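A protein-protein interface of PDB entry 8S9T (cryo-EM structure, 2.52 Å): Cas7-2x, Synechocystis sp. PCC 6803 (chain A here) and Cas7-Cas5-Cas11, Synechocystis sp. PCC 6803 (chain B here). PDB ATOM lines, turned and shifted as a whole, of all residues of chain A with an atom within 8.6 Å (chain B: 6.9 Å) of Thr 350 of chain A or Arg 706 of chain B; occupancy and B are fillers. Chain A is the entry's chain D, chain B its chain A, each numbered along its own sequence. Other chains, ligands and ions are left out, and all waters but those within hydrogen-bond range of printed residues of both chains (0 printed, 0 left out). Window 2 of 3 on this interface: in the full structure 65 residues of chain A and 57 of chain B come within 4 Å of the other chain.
The guanidinium group (NH2) of Arg 706 of chain B lies within hydrogen-bond range of the backbone carbonyl oxygen (O) of Thr 350 of chain A (2.5 Å).
The guanidinium group (NH2) of Arg 706 of chain B lies within hydrogen-bond range of the backbone carbonyl oxygen (O) of Leu 243 of chain A (3.0 Å).
N of Lys 707 of chain B lies within hydrogen-bond range of O of Leu 700 of chain B.
The backbone carbonyl oxygen (O) of Ala 699 of chain B lies within hydrogen-bond range of the guanidinium group (NH1) of Arg 706 of chain B (2.9 Å).
The backbone NH (N) of Thr 350 of chain A lies within hydrogen-bond range of the side-chain amide oxygen (OD1) of Asn 355 of chain A, at 2.8 Å.
Printed residues of chain B within 4 Å of Leu 243 of chain A: Tyr 696, Ala 699, Leu 700 and Arg 706.
Asn 355 of chain A touches none of the printed residues of chain B.
Printed residues of chain A within 4 Å of Tyr 696 of chain B: Leu 243.
Of the printed residues of chain A, Ala 699 of chain B touches Leu 243 (3.7 Å) and Thr 350 (3.6 Å).
No residue of chain A comes within 4 Å of Asn 705 of chain B.
Arg 706 of chain B touches two residues of chain A.
The nearest printed residue of chain A that does not touch Tyr 696 of chain B is Asp 241 of chain A (4.7 Å).
Among the printed residues, merely in contact across the chains: Thr 350 of chain A with Ala 699 of chain B, Leu 243 of chain A with Ala 699 of chain B, Leu 243 of chain A with Tyr 696 of chain B and Leu 243 of chain A with Leu 700 of chain B.
Hydrophobic or aromatic side chains of chain B that line the printed part of chain A: Tyr 696, Ala 699 and Leu 700.
Hydrophobic or aromatic side chains of chain A within 4 Å of the printed part of chain B: Leu 243.
Among the printed residues, 6 pairs touch across the chains.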
ATOM      1  N   ASP A 241      20.411 -14.532 -26.550  1.00  0.00           N
ATOM      2  CA  ASP A 241      20.032 -15.616 -27.441  1.00  0.00           C
ATOM      3  C   ASP A 241      18.959 -16.474 -26.798  1.00  0.00           C
ATOM      4  O   ASP A 241      18.952 -16.686 -25.585  1.00  0.00           O
ATOM      5  CB  ASP A 241      21.232 -16.487 -27.798  1.00  0.00           C
ATOM      6  CG  ASP A 241      22.172 -15.819 -28.764  1.00  0.00           C
ATOM      7  OD1 ASP A 241      21.787 -14.792 -29.364  1.00  0.00           O
ATOM      8  OD2 ASP A 241      23.286 -16.349 -28.957  1.00  0.00           O
ATOM      9  N   GLY A 242      18.039 -16.957 -27.617  1.00  0.00           N
ATOM     10  CA  GLY A 242      17.181 -18.045 -27.223  1.00  0.00           C
ATOM     11  C   GLY A 242      17.880 -19.375 -27.374  1.00  0.00           C
ATOM     12  O   GLY A 242      19.041 -19.470 -27.763  1.00  0.00           O
ATOM     13  N   LEU A 243      17.141 -20.430 -27.058  1.00  0.00           N
ATOM     14  CA  LEU A 243      17.663 -21.781 -27.156  1.00  0.00           C
ATOM     15  C   LEU A 243      17.491 -22.346 -28.558  1.00  0.00           C
ATOM     16  O   LEU A 243      18.464 -22.794 -29.167  1.00  0.00           O
ATOM     17  CB  LEU A 243      16.975 -22.683 -26.131  1.00  0.00           C
ATOM     18  CG  LEU A 243      17.412 -22.554 -24.679  1.00  0.00           C
ATOM     19  CD1 LEU A 243      16.395 -23.204 -23.785  1.00  0.00           C
ATOM     20  CD2 LEU A 243      18.761 -23.206 -24.502  1.00  0.00           C
ATOM     21  N   ALA A 244      16.271 -22.329 -29.087  1.00  0.00           N
ATOM     22  CA  ALA A 244      16.094 -22.690 -30.482  1.00  0.00           C
ATOM     23  C   ALA A 244      16.554 -21.581 -31.417  1.00  0.00           C
ATOM     24  O   ALA A 244      17.213 -21.856 -32.423  1.00  0.00           O
ATOM     25  CB  ALA A 244      14.635 -23.035 -30.752  1.00  0.00           C
ATOM     26  N   ILE A 245      16.223 -20.332 -31.113  1.00  0.00           N
ATOM     27  CA  ILE A 245      16.556 -19.192 -31.955  1.00  0.00           C
ATOM     28  C   ILE A 245      17.676 -18.401 -31.303  1.00  0.00           C
ATOM     29  O   ILE A 245      17.564 -18.014 -30.140  1.00  0.00           O
ATOM     30  CB  ILE A 245      15.330 -18.301 -32.200  1.00  0.00           C
ATOM     31  CG1 ILE A 245      14.217 -19.090 -32.870  1.00  0.00           C
ATOM     32  CG2 ILE A 245      15.711 -17.161 -33.071  1.00  0.00           C
ATOM     33  CD1 ILE A 245      14.560 -19.530 -34.242  1.00  0.00           C
ATOM     34  N   ASP A 246      18.727 -18.106 -32.059  1.00  0.00           N
ATOM     35  CA  ASP A 246      19.739 -17.181 -31.563  1.00  0.00           C
ATOM     36  C   ASP A 246      19.195 -15.766 -31.452  1.00  0.00           C
ATOM     37  O   ASP A 246      19.112 -15.207 -30.359  1.00  0.00           O
ATOM     38  CB  ASP A 246      20.964 -17.197 -32.467  1.00  0.00           C
ATOM     39  CG  ASP A 246      21.485 -18.571 -32.705  1.00  0.00           C
ATOM     40  OD1 ASP A 246      21.318 -19.436 -31.828  1.00  0.00           O
ATOM     41  OD2 ASP A 246      22.093 -18.786 -33.760  1.00  0.00           O
ATOM     42  N   LYS A 344       7.426 -16.349 -23.130  1.00  0.00           N
ATOM     43  CA  LYS A 344       8.393 -17.200 -22.441  1.00  0.00           C
ATOM     44  C   LYS A 344       8.434 -18.590 -23.051  1.00  0.00           C
ATOM     45  O   LYS A 344       9.498 -19.208 -23.121  1.00  0.00           O
ATOM     46  CB  LYS A 344       8.084 -17.291 -20.948  1.00  0.00           C
ATOM     47  CG  LYS A 344       8.030 -15.979 -20.188  1.00  0.00           C
ATOM     48  CD  LYS A 344       8.982 -14.948 -20.766  1.00  0.00           C
ATOM     49  CE  LYS A 344       8.863 -13.619 -20.043  1.00  0.00           C
ATOM     50  NZ  LYS A 344       9.703 -12.570 -20.682  1.00  0.00           N
ATOM     51  N   ALA A 345       7.284 -19.105 -23.487  1.00  0.00           N
ATOM     52  CA  ALA A 345       7.267 -20.389 -24.176  1.00  0.00           C
ATOM     53  C   ALA A 345       8.104 -20.360 -25.448  1.00  0.00           C
ATOM     54  O   ALA A 345       8.731 -21.360 -25.805  1.00  0.00           O
ATOM     55  CB  ALA A 345       5.830 -20.787 -24.495  1.00  0.00           C
ATOM     56  N   VAL A 346       8.118 -19.229 -26.150  1.00  0.00           N
ATOM     57  CA  VAL A 346       8.990 -19.072 -27.309  1.00  0.00           C
ATOM     58  C   VAL A 346      10.447 -18.946 -26.878  1.00  0.00           C
ATOM     59  O   VAL A 346      11.336 -19.573 -27.462  1.00  0.00           O
ATOM     60  CB  VAL A 346       8.542 -17.873 -28.164  1.00  0.00           C
ATOM     61  CG1 VAL A 346       9.454 -17.709 -29.352  1.00  0.00           C
ATOM     62  CG2 VAL A 346       7.133 -18.089 -28.653  1.00  0.00           C
ATOM     63  N   GLU A 347      10.720 -18.107 -25.875  1.00  0.00           N
ATOM     64  CA  GLU A 347      12.091 -17.940 -25.402  1.00  0.00           C
ATOM     65  C   GLU A 347      12.676 -19.242 -24.874  1.00  0.00           C
ATOM     66  O   GLU A 347      13.864 -19.520 -25.066  1.00  0.00           O
ATOM     67  CB  GLU A 347      12.153 -16.882 -24.309  1.00  0.00           C
ATOM     68  CG  GLU A 347      11.769 -15.497 -24.721  1.00  0.00           C
ATOM     69  CD  GLU A 347      12.043 -14.508 -23.622  1.00  0.00           C
ATOM     70  OE1 GLU A 347      12.037 -14.923 -22.448  1.00  0.00           O
ATOM     71  OE2 GLU A 347      12.284 -13.322 -23.919  1.00  0.00           O
ATOM     72  N   ASN A 348      11.864 -20.048 -24.200  1.00  0.00           N
ATOM     73  CA  ASN A 348      12.349 -21.293 -23.629  1.00  0.00           C
ATOM     74  C   ASN A 348      12.445 -22.406 -24.652  1.00  0.00           C
ATOM     75  O   ASN A 348      13.086 -23.421 -24.375  1.00  0.00           O
ATOM     76  CB  ASN A 348      11.447 -21.725 -22.479  1.00  0.00           C
ATOM     77  CG  ASN A 348      11.472 -20.750 -21.327  1.00  0.00           C
ATOM     78  OD1 ASN A 348      12.364 -19.909 -21.230  1.00  0.00           O
ATOM     79  ND2 ASN A 348      10.475 -20.838 -20.459  1.00  0.00           N
ATOM     80  N   ALA A 349      11.809 -22.248 -25.808  1.00  0.00           N
ATOM     81  CA  ALA A 349      11.744 -23.320 -26.789  1.00  0.00           C
ATOM     82  C   ALA A 349      13.141 -23.793 -27.160  1.00  0.00           C
ATOM     83  O   ALA A 349      14.011 -22.994 -27.512  1.00  0.00           O
ATOM     84  CB  ALA A 349      10.997 -22.846 -28.025  1.00  0.00           C
ATOM     85  N   THR A 350      13.360 -25.096 -27.035  1.00  0.00           N
ATOM     86  CA  THR A 350      14.670 -25.705 -27.211  1.00  0.00           C
ATOM     87  C   THR A 350      14.906 -26.254 -28.608  1.00  0.00           C
ATOM     88  O   THR A 350      16.062 -26.437 -28.993  1.00  0.00           O
ATOM     89  CB  THR A 350      14.876 -26.823 -26.178  1.00  0.00           C
ATOM     90  OG1 THR A 350      14.021 -27.931 -26.481  1.00  0.00           O
ATOM     91  CG2 THR A 350      14.563 -26.330 -24.784  1.00  0.00           C
ATOM     92  N   GLU A 351      13.854 -26.512 -29.375  1.00  0.00           N
ATOM     93  CA  GLU A 351      13.968 -27.176 -30.664  1.00  0.00           C
ATOM     94  C   GLU A 351      13.155 -26.432 -31.707  1.00  0.00           C
ATOM     95  O   GLU A 351      11.959 -26.211 -31.518  1.00  0.00           O
ATOM     96  CB  GLU A 351      13.463 -28.614 -30.571  1.00  0.00           C
ATOM     97  CG  GLU A 351      14.325 -29.534 -29.763  1.00  0.00           C
ATOM     98  CD  GLU A 351      13.827 -30.957 -29.813  1.00  0.00           C
ATOM     99  OE1 GLU A 351      14.659 -31.884 -29.929  1.00  0.00           O
ATOM    100  OE2 GLU A 351      12.595 -31.146 -29.723  1.00  0.00           O
ATOM    101  N   MET A 352      13.813 -26.050 -32.804  1.00  0.00           N
ATOM    102  CA  MET A 352      13.171 -25.196 -33.793  1.00  0.00           C
ATOM    103  C   MET A 352      11.972 -25.879 -34.434  1.00  0.00           C
ATOM    104  O   MET A 352      10.946 -25.240 -34.684  1.00  0.00           O
ATOM    105  CB  MET A 352      14.183 -24.784 -34.854  1.00  0.00           C
ATOM    106  CG  MET A 352      13.568 -24.076 -36.041  1.00  0.00           C
ATOM    107  SD  MET A 352      14.763 -23.570 -37.271  1.00  0.00           S
ATOM    108  CE  MET A 352      15.473 -22.171 -36.429  1.00  0.00           C
ATOM    109  N   THR A 353      12.070 -27.176 -34.692  1.00  0.00           N
ATOM    110  CA  THR A 353      10.943 -27.943 -35.189  1.00  0.00           C
ATOM    111  C   THR A 353      10.294 -28.762 -34.098  1.00  0.00           C
ATOM    112  O   THR A 353       9.351 -29.508 -34.369  1.00  0.00           O
ATOM    113  CB  THR A 353      11.367 -28.860 -36.343  1.00  0.00           C
ATOM    114  OG1 THR A 353      12.495 -29.647 -35.948  1.00  0.00           O
ATOM    115  CG2 THR A 353      11.717 -28.050 -37.571  1.00  0.00           C
ATOM    116  N   GLY A 354      10.773 -28.629 -32.874  1.00  0.00           N
ATOM    117  CA  GLY A 354      10.104 -29.185 -31.729  1.00  0.00           C
ATOM    118  C   GLY A 354       9.196 -28.182 -31.071  1.00  0.00           C
ATOM    119  O   GLY A 354       8.294 -27.641 -31.703  1.00  0.00           O
ATOM    120  N   ASN A 355       9.392 -27.978 -29.774  1.00  0.00           N
ATOM    121  CA  ASN A 355       8.486 -27.181 -28.966  1.00  0.00           C
ATOM    122  C   ASN A 355       8.418 -25.712 -29.368  1.00  0.00           C
ATOM    123  O   ASN A 355       7.552 -25.001 -28.857  1.00  0.00           O
ATOM    124  CB  ASN A 355       8.873 -27.357 -27.502  1.00  0.00           C
ATOM    125  CG  ASN A 355      10.337 -27.113 -27.252  1.00  0.00           C
ATOM    126  OD1 ASN A 355      10.947 -26.248 -27.857  1.00  0.00           O
ATOM    127  ND2 ASN A 355      10.918 -27.906 -26.372  1.00  0.00           N
ATOM    128  N   LEU A 356       9.283 -25.243 -30.271  1.00  0.00           N
ATOM    129  CA  LEU A 356       9.133 -23.895 -30.817  1.00  0.00           C
ATOM    130  C   LEU A 356       7.887 -23.745 -31.675  1.00  0.00           C
ATOM    131  O   LEU A 356       7.250 -22.691 -31.664  1.00  0.00           O
ATOM    132  CB  LEU A 356      10.367 -23.519 -31.631  1.00  0.00           C
ATOM    133  CG  LEU A 356      10.397 -22.116 -32.236  1.00  0.00           C
ATOM    134  CD1 LEU A 356      10.586 -21.060 -31.170  1.00  0.00           C
ATOM    135  CD2 LEU A 356      11.471 -22.008 -33.289  1.00  0.00           C
ATOM    136  N   GLN A 357       7.514 -24.780 -32.419  1.00  0.00           N
ATOM    137  CA  GLN A 357       6.339 -24.658 -33.279  1.00  0.00           C
ATOM    138  C   GLN A 357       5.044 -24.486 -32.499  1.00  0.00           C
ATOM    139  O   GLN A 357       4.235 -23.630 -32.886  1.00  0.00           O
ATOM    140  CB  GLN A 357       6.283 -25.834 -34.257  1.00  0.00           C
ATOM    141  CG  GLN A 357       7.566 -26.061 -35.002  1.00  0.00           C
ATOM    142  CD  GLN A 357       7.380 -26.969 -36.184  1.00  0.00           C
ATOM    143  OE1 GLN A 357       6.453 -27.775 -36.219  1.00  0.00           O
ATOM    144  NE2 GLN A 357       8.248 -26.840 -37.173  1.00  0.00           N
ATOM    145  N   ALA A 359       4.908 -23.108 -29.485  1.00  0.00           N
ATOM    146  CA  ALA A 359       5.080 -21.803 -28.871  1.00  0.00           C
ATOM    147  C   ALA A 359       4.848 -20.667 -29.856  1.00  0.00           C
ATOM    148  O   ALA A 359       4.278 -19.636 -29.487  1.00  0.00           O
ATOM    149  CB  ALA A 359       6.471 -21.701 -28.253  1.00  0.00           C
ATOM    150  N   GLN B 673      25.415 -15.598 -24.610  1.00  0.00           N
ATOM    151  CA  GLN B 673      25.075 -16.632 -23.643  1.00  0.00           C
ATOM    152  C   GLN B 673      24.807 -16.035 -22.269  1.00  0.00           C
ATOM    153  O   GLN B 673      23.911 -16.490 -21.552  1.00  0.00           O
ATOM    154  CB  GLN B 673      26.185 -17.673 -23.569  1.00  0.00           C
ATOM    155  CG  GLN B 673      26.291 -18.538 -24.797  1.00  0.00           C
ATOM    156  CD  GLN B 673      25.085 -19.430 -24.973  1.00  0.00           C
ATOM    157  OE1 GLN B 673      24.123 -19.063 -25.642  1.00  0.00           O
ATOM    158  NE2 GLN B 673      25.118 -20.599 -24.350  1.00  0.00           N
ATOM    159  N   GLY B 695      15.751 -25.481 -15.170  1.00  0.00           N
ATOM    160  CA  GLY B 695      15.233 -25.972 -16.437  1.00  0.00           C
ATOM    161  C   GLY B 695      16.025 -25.474 -17.629  1.00  0.00           C
ATOM    162  O   GLY B 695      16.418 -26.249 -18.499  1.00  0.00           O
ATOM    163  N   TYR B 696      16.253 -24.164 -17.687  1.00  0.00           N
ATOM    164  CA  TYR B 696      17.046 -23.585 -18.766  1.00  0.00           C
ATOM    165  C   TYR B 696      18.445 -24.185 -18.831  1.00  0.00           C
ATOM    166  O   TYR B 696      18.946 -24.483 -19.921  1.00  0.00           O
ATOM    167  CB  TYR B 696      17.107 -22.068 -18.597  1.00  0.00           C
ATOM    168  CG  TYR B 696      18.045 -21.386 -19.556  1.00  0.00           C
ATOM    169  CD1 TYR B 696      17.670 -21.144 -20.863  1.00  0.00           C
ATOM    170  CD2 TYR B 696      19.294 -20.963 -19.147  1.00  0.00           C
ATOM    171  CE1 TYR B 696      18.513 -20.515 -21.731  1.00  0.00           C
ATOM    172  CE2 TYR B 696      20.142 -20.339 -20.011  1.00  0.00           C
ATOM    173  CZ  TYR B 696      19.750 -20.116 -21.301  1.00  0.00           C
ATOM    174  OH  TYR B 696      20.610 -19.495 -22.173  1.00  0.00           O
ATOM    175  N   THR B 698      19.348 -27.133 -17.933  1.00  0.00           N
ATOM    176  CA  THR B 698      19.247 -28.473 -18.502  1.00  0.00           C
ATOM    177  C   THR B 698      19.282 -28.430 -20.024  1.00  0.00           C
ATOM    178  O   THR B 698      20.032 -29.177 -20.662  1.00  0.00           O
ATOM    179  CB  THR B 698      17.965 -29.152 -18.020  1.00  0.00           C
ATOM    180  OG1 THR B 698      17.911 -29.126 -16.591  1.00  0.00           O
ATOM    181  CG2 THR B 698      17.908 -30.586 -18.501  1.00  0.00           C
ATOM    182  N   ALA B 699      18.477 -27.554 -20.624  1.00  0.00           N
ATOM    183  CA  ALA B 699      18.450 -27.421 -22.074  1.00  0.00           C
ATOM    184  C   ALA B 699      19.747 -26.855 -22.646  1.00  0.00           C
ATOM    185  O   ALA B 699      20.072 -27.133 -23.802  1.00  0.00           O
ATOM    186  CB  ALA B 699      17.273 -26.547 -22.480  1.00  0.00           C
ATOM    187  N   LEU B 700      20.510 -26.081 -21.872  1.00  0.00           N
ATOM    188  CA  LEU B 700      21.847 -25.700 -22.321  1.00  0.00           C
ATOM    189  C   LEU B 700      22.764 -26.907 -22.428  1.00  0.00           C
ATOM    190  O   LEU B 700      23.333 -27.183 -23.490  1.00  0.00           O
ATOM    191  CB  LEU B 700      22.463 -24.674 -21.372  1.00  0.00           C
ATOM    192  CG  LEU B 700      22.008 -23.226 -21.382  1.00  0.00           C
ATOM    193  CD1 LEU B 700      22.762 -22.479 -20.302  1.00  0.00           C
ATOM    194  CD2 LEU B 700      22.281 -22.618 -22.728  1.00  0.00           C
ATOM    195  N   GLU B 701      22.920 -27.636 -21.335  1.00  0.00           N
ATOM    196  CA  GLU B 701      23.858 -28.743 -21.286  1.00  0.00           C
ATOM    197  C   GLU B 701      23.319 -29.986 -21.974  1.00  0.00           C
ATOM    198  O   GLU B 701      24.070 -30.947 -22.167  1.00  0.00           O
ATOM    199  CB  GLU B 701      24.235 -29.027 -19.830  1.00  0.00           C
ATOM    200  CG  GLU B 701      23.116 -29.587 -18.991  1.00  0.00           C
ATOM    201  CD  GLU B 701      23.381 -29.428 -17.512  1.00  0.00           C
ATOM    202  OE1 GLU B 701      24.534 -29.646 -17.090  1.00  0.00           O
ATOM    203  OE2 GLU B 701      22.439 -29.085 -16.770  1.00  0.00           O
ATOM    204  N   GLN B 702      22.042 -29.979 -22.351  1.00  0.00           N
ATOM    205  CA  GLN B 702      21.466 -31.096 -23.088  1.00  0.00           C
ATOM    206  C   GLN B 702      22.088 -31.259 -24.473  1.00  0.00           C
ATOM    207  O   GLN B 702      22.117 -32.375 -25.002  1.00  0.00           O
ATOM    208  CB  GLN B 702      19.956 -30.900 -23.212  1.00  0.00           C
ATOM    209  CG  GLN B 702      19.231 -31.988 -23.957  1.00  0.00           C
ATOM    210  CD  GLN B 702      17.735 -31.808 -23.921  1.00  0.00           C
ATOM    211  OE1 GLN B 702      17.238 -30.696 -23.749  1.00  0.00           O
ATOM    212  NE2 GLN B 702      17.002 -32.905 -24.073  1.00  0.00           N
ATOM    213  N   VAL B 703      22.599 -30.184 -25.074  1.00  0.00           N
ATOM    214  CA  VAL B 703      23.022 -30.213 -26.471  1.00  0.00           C
ATOM    215  C   VAL B 703      24.421 -29.627 -26.597  1.00  0.00           C
ATOM    216  O   VAL B 703      24.729 -28.588 -26.002  1.00  0.00           O
ATOM    217  CB  VAL B 703      22.044 -29.451 -27.391  1.00  0.00           C
ATOM    218  CG1 VAL B 703      22.301 -29.820 -28.844  1.00  0.00           C
ATOM    219  CG2 VAL B 703      20.606 -29.729 -27.010  1.00  0.00           C
ATOM    220  N   SER B 704      25.269 -30.314 -27.367  1.00  0.00           N
ATOM    221  CA  SER B 704      26.689 -29.982 -27.439  1.00  0.00           C
ATOM    222  C   SER B 704      26.929 -28.559 -27.929  1.00  0.00           C
ATOM    223  O   SER B 704      27.814 -27.865 -27.418  1.00  0.00           O
ATOM    224  CB  SER B 704      27.409 -30.982 -28.343  1.00  0.00           C
ATOM    225  OG  SER B 704      27.184 -32.313 -27.916  1.00  0.00           O
ATOM    226  N   ASN B 705      26.168 -28.114 -28.934  1.00  0.00           N
ATOM    227  CA  ASN B 705      26.391 -26.788 -29.504  1.00  0.00           C
ATOM    228  C   ASN B 705      26.240 -25.689 -28.460  1.00  0.00           C
ATOM    229  O   ASN B 705      26.944 -24.676 -28.516  1.00  0.00           O
ATOM    230  CB  ASN B 705      25.430 -26.563 -30.672  1.00  0.00           C
ATOM    231  CG  ASN B 705      23.974 -26.553 -30.240  1.00  0.00           C
ATOM    232  OD1 ASN B 705      23.643 -26.961 -29.126  1.00  0.00           O
ATOM    233  ND2 ASN B 705      23.096 -26.101 -31.125  1.00  0.00           N
ATOM    234  N   ARG B 706      25.348 -25.885 -27.495  1.00  0.00           N
ATOM    235  CA  ARG B 706      25.199 -24.958 -26.382  1.00  0.00           C
ATOM    236  C   ARG B 706      26.226 -25.271 -25.307  1.00  0.00           C
ATOM    237  O   ARG B 706      26.898 -24.373 -24.788  1.00  0.00           O
ATOM    238  CB  ARG B 706      23.792 -25.069 -25.806  1.00  0.00           C
ATOM    239  CG  ARG B 706      22.682 -24.654 -26.746  1.00  0.00           C
ATOM    240  CD  ARG B 706      21.354 -25.249 -26.295  1.00  0.00           C
ATOM    241  NE  ARG B 706      20.323 -25.124 -27.319  1.00  0.00           N
ATOM    242  CZ  ARG B 706      19.284 -25.941 -27.449  1.00  0.00           C
ATOM    243  NH1 ARG B 706      19.038 -26.863 -26.535  1.00  0.00           N
ATOM    244  NH2 ARG B 706      18.417 -25.747 -28.426  1.00  0.00           N
ATOM    245  N   LYS B 707      26.341 -26.555 -24.968  1.00  0.00           N
ATOM    246  CA  LYS B 707      27.275 -27.013 -23.949  1.00  0.00           C
ATOM    247  C   LYS B 707      28.702 -26.575 -24.250  1.00  0.00           C
ATOM    248  O   LYS B 707      29.450 -26.217 -23.335  1.00  0.00           O
ATOM    249  CB  LYS B 707      27.185 -28.535 -23.855  1.00  0.00           C
ATOM    250  CG  LYS B 707      28.116 -29.207 -22.876  1.00  0.00           C
ATOM    251  CD  LYS B 707      27.722 -28.858 -21.463  1.00  0.00           C
ATOM    252  CE  LYS B 707      28.525 -29.647 -20.450  1.00  0.00           C
ATOM    253  NZ  LYS B 707      27.992 -29.420 -19.081  1.00  0.00           N
ATOM    254  N   GLU B 708      29.101 -26.597 -25.521  1.00  0.00           N
ATOM    255  CA  GLU B 708      30.469 -26.236 -25.877  1.00  0.00           C
ATOM    256  C   GLU B 708      30.771 -24.759 -25.669  1.00  0.00           C
ATOM    257  O   GLU B 708      31.943 -24.397 -25.530  1.00  0.00           O
ATOM    258  CB  GLU B 708      30.776 -26.608 -27.326  1.00  0.00           C
ATOM    259  CG  GLU B 708      30.183 -25.678 -28.364  1.00  0.00           C
ATOM    260  CD  GLU B 708      30.672 -25.996 -29.761  1.00  0.00           C
ATOM    261  OE1 GLU B 708      31.139 -25.069 -30.454  1.00  0.00           O
ATOM    262  OE2 GLU B 708      30.596 -27.177 -30.164  1.00  0.00           O
ATOM    263  N   LYS B 709      29.756 -23.895 -25.670  1.00  0.00           N
ATOM    264  CA  LYS B 709      30.007 -22.471 -25.466  1.00  0.00           C
ATOM    265  C   LYS B 709      30.399 -22.182 -24.025  1.00  0.00           C
ATOM    266  O   LYS B 709      31.332 -21.416 -23.768  1.00  0.00           O
ATOM    267  CB  LYS B 709      28.761 -21.675 -25.843  1.00  0.00           C
ATOM    268  CG  LYS B 709      28.165 -22.058 -27.186  1.00  0.00           C
ATOM    269  CD  LYS B 709      27.058 -21.111 -27.608  1.00  0.00           C
ATOM    270  CE  LYS B 709      27.595 -19.804 -28.165  1.00  0.00           C
ATOM    271  NZ  LYS B 709      28.167 -19.972 -29.535  1.00  0.00           N
ATOM    272  N   TRP B 710      29.704 -22.799 -23.077  1.00  0.00           N
ATOM    273  CA  TRP B 710      30.029 -22.699 -21.660  1.00  0.00           C
ATOM    274  C   TRP B 710      31.204 -23.570 -21.238  1.00  0.00           C
ATOM    275  O   TRP B 710      31.767 -23.341 -20.166  1.00  0.00           O
ATOM    276  CB  TRP B 710      28.791 -23.049 -20.841  1.00  0.00           C
ATOM    277  CG  TRP B 710      27.801 -21.943 -20.795  1.00  0.00           C
ATOM    278  CD1 TRP B 710      26.717 -21.785 -21.595  1.00  0.00           C
ATOM    279  CD2 TRP B 710      27.753 -20.883 -19.839  1.00  0.00           C
ATOM    280  NE1 TRP B 710      26.023 -20.660 -21.237  1.00  0.00           N
ATOM    281  CE2 TRP B 710      26.635 -20.091 -20.152  1.00  0.00           C
ATOM    282  CE3 TRP B 710      28.558 -20.516 -18.757  1.00  0.00           C
ATOM    283  CZ2 TRP B 710      26.297 -18.957 -19.424  1.00  0.00           C
ATOM    284  CZ3 TRP B 710      28.227 -19.396 -18.039  1.00  0.00           C
ATOM    285  CH2 TRP B 710      27.106 -18.625 -18.375  1.00  0.00           C
ATOM    286  N   SER B 711      31.564 -24.583 -22.022  1.00  0.00           N
ATOM    287  CA  SER B 711      32.591 -25.517 -21.580  1.00  0.00           C
ATOM    288  C   SER B 711      33.972 -24.889 -21.484  1.00  0.00           C
ATOM    289  O   SER B 711      34.852 -25.466 -20.837  1.00  0.00           O
ATOM    290  CB  SER B 711      32.636 -26.727 -22.509  1.00  0.00           C
ATOM    291  OG  SER B 711      31.462 -27.503 -22.368  1.00  0.00           O
ATOM    292  N   LEU B 717      28.264 -23.688 -15.746  1.00  0.00           N
ATOM    293  CA  LEU B 717      26.898 -24.204 -15.677  1.00  0.00           C
ATOM    294  C   LEU B 717      26.601 -24.944 -14.380  1.00  0.00           C
ATOM    295  O   LEU B 717      25.454 -24.935 -13.926  1.00  0.00           O
ATOM    296  CB  LEU B 717      26.600 -25.090 -16.876  1.00  0.00           C
ATOM    297  CG  LEU B 717      26.627 -24.315 -18.185  1.00  0.00           C
ATOM    298  CD1 LEU B 717      26.214 -25.213 -19.336  1.00  0.00           C
ATOM    299  CD2 LEU B 717      25.727 -23.103 -18.079  1.00  0.00           C
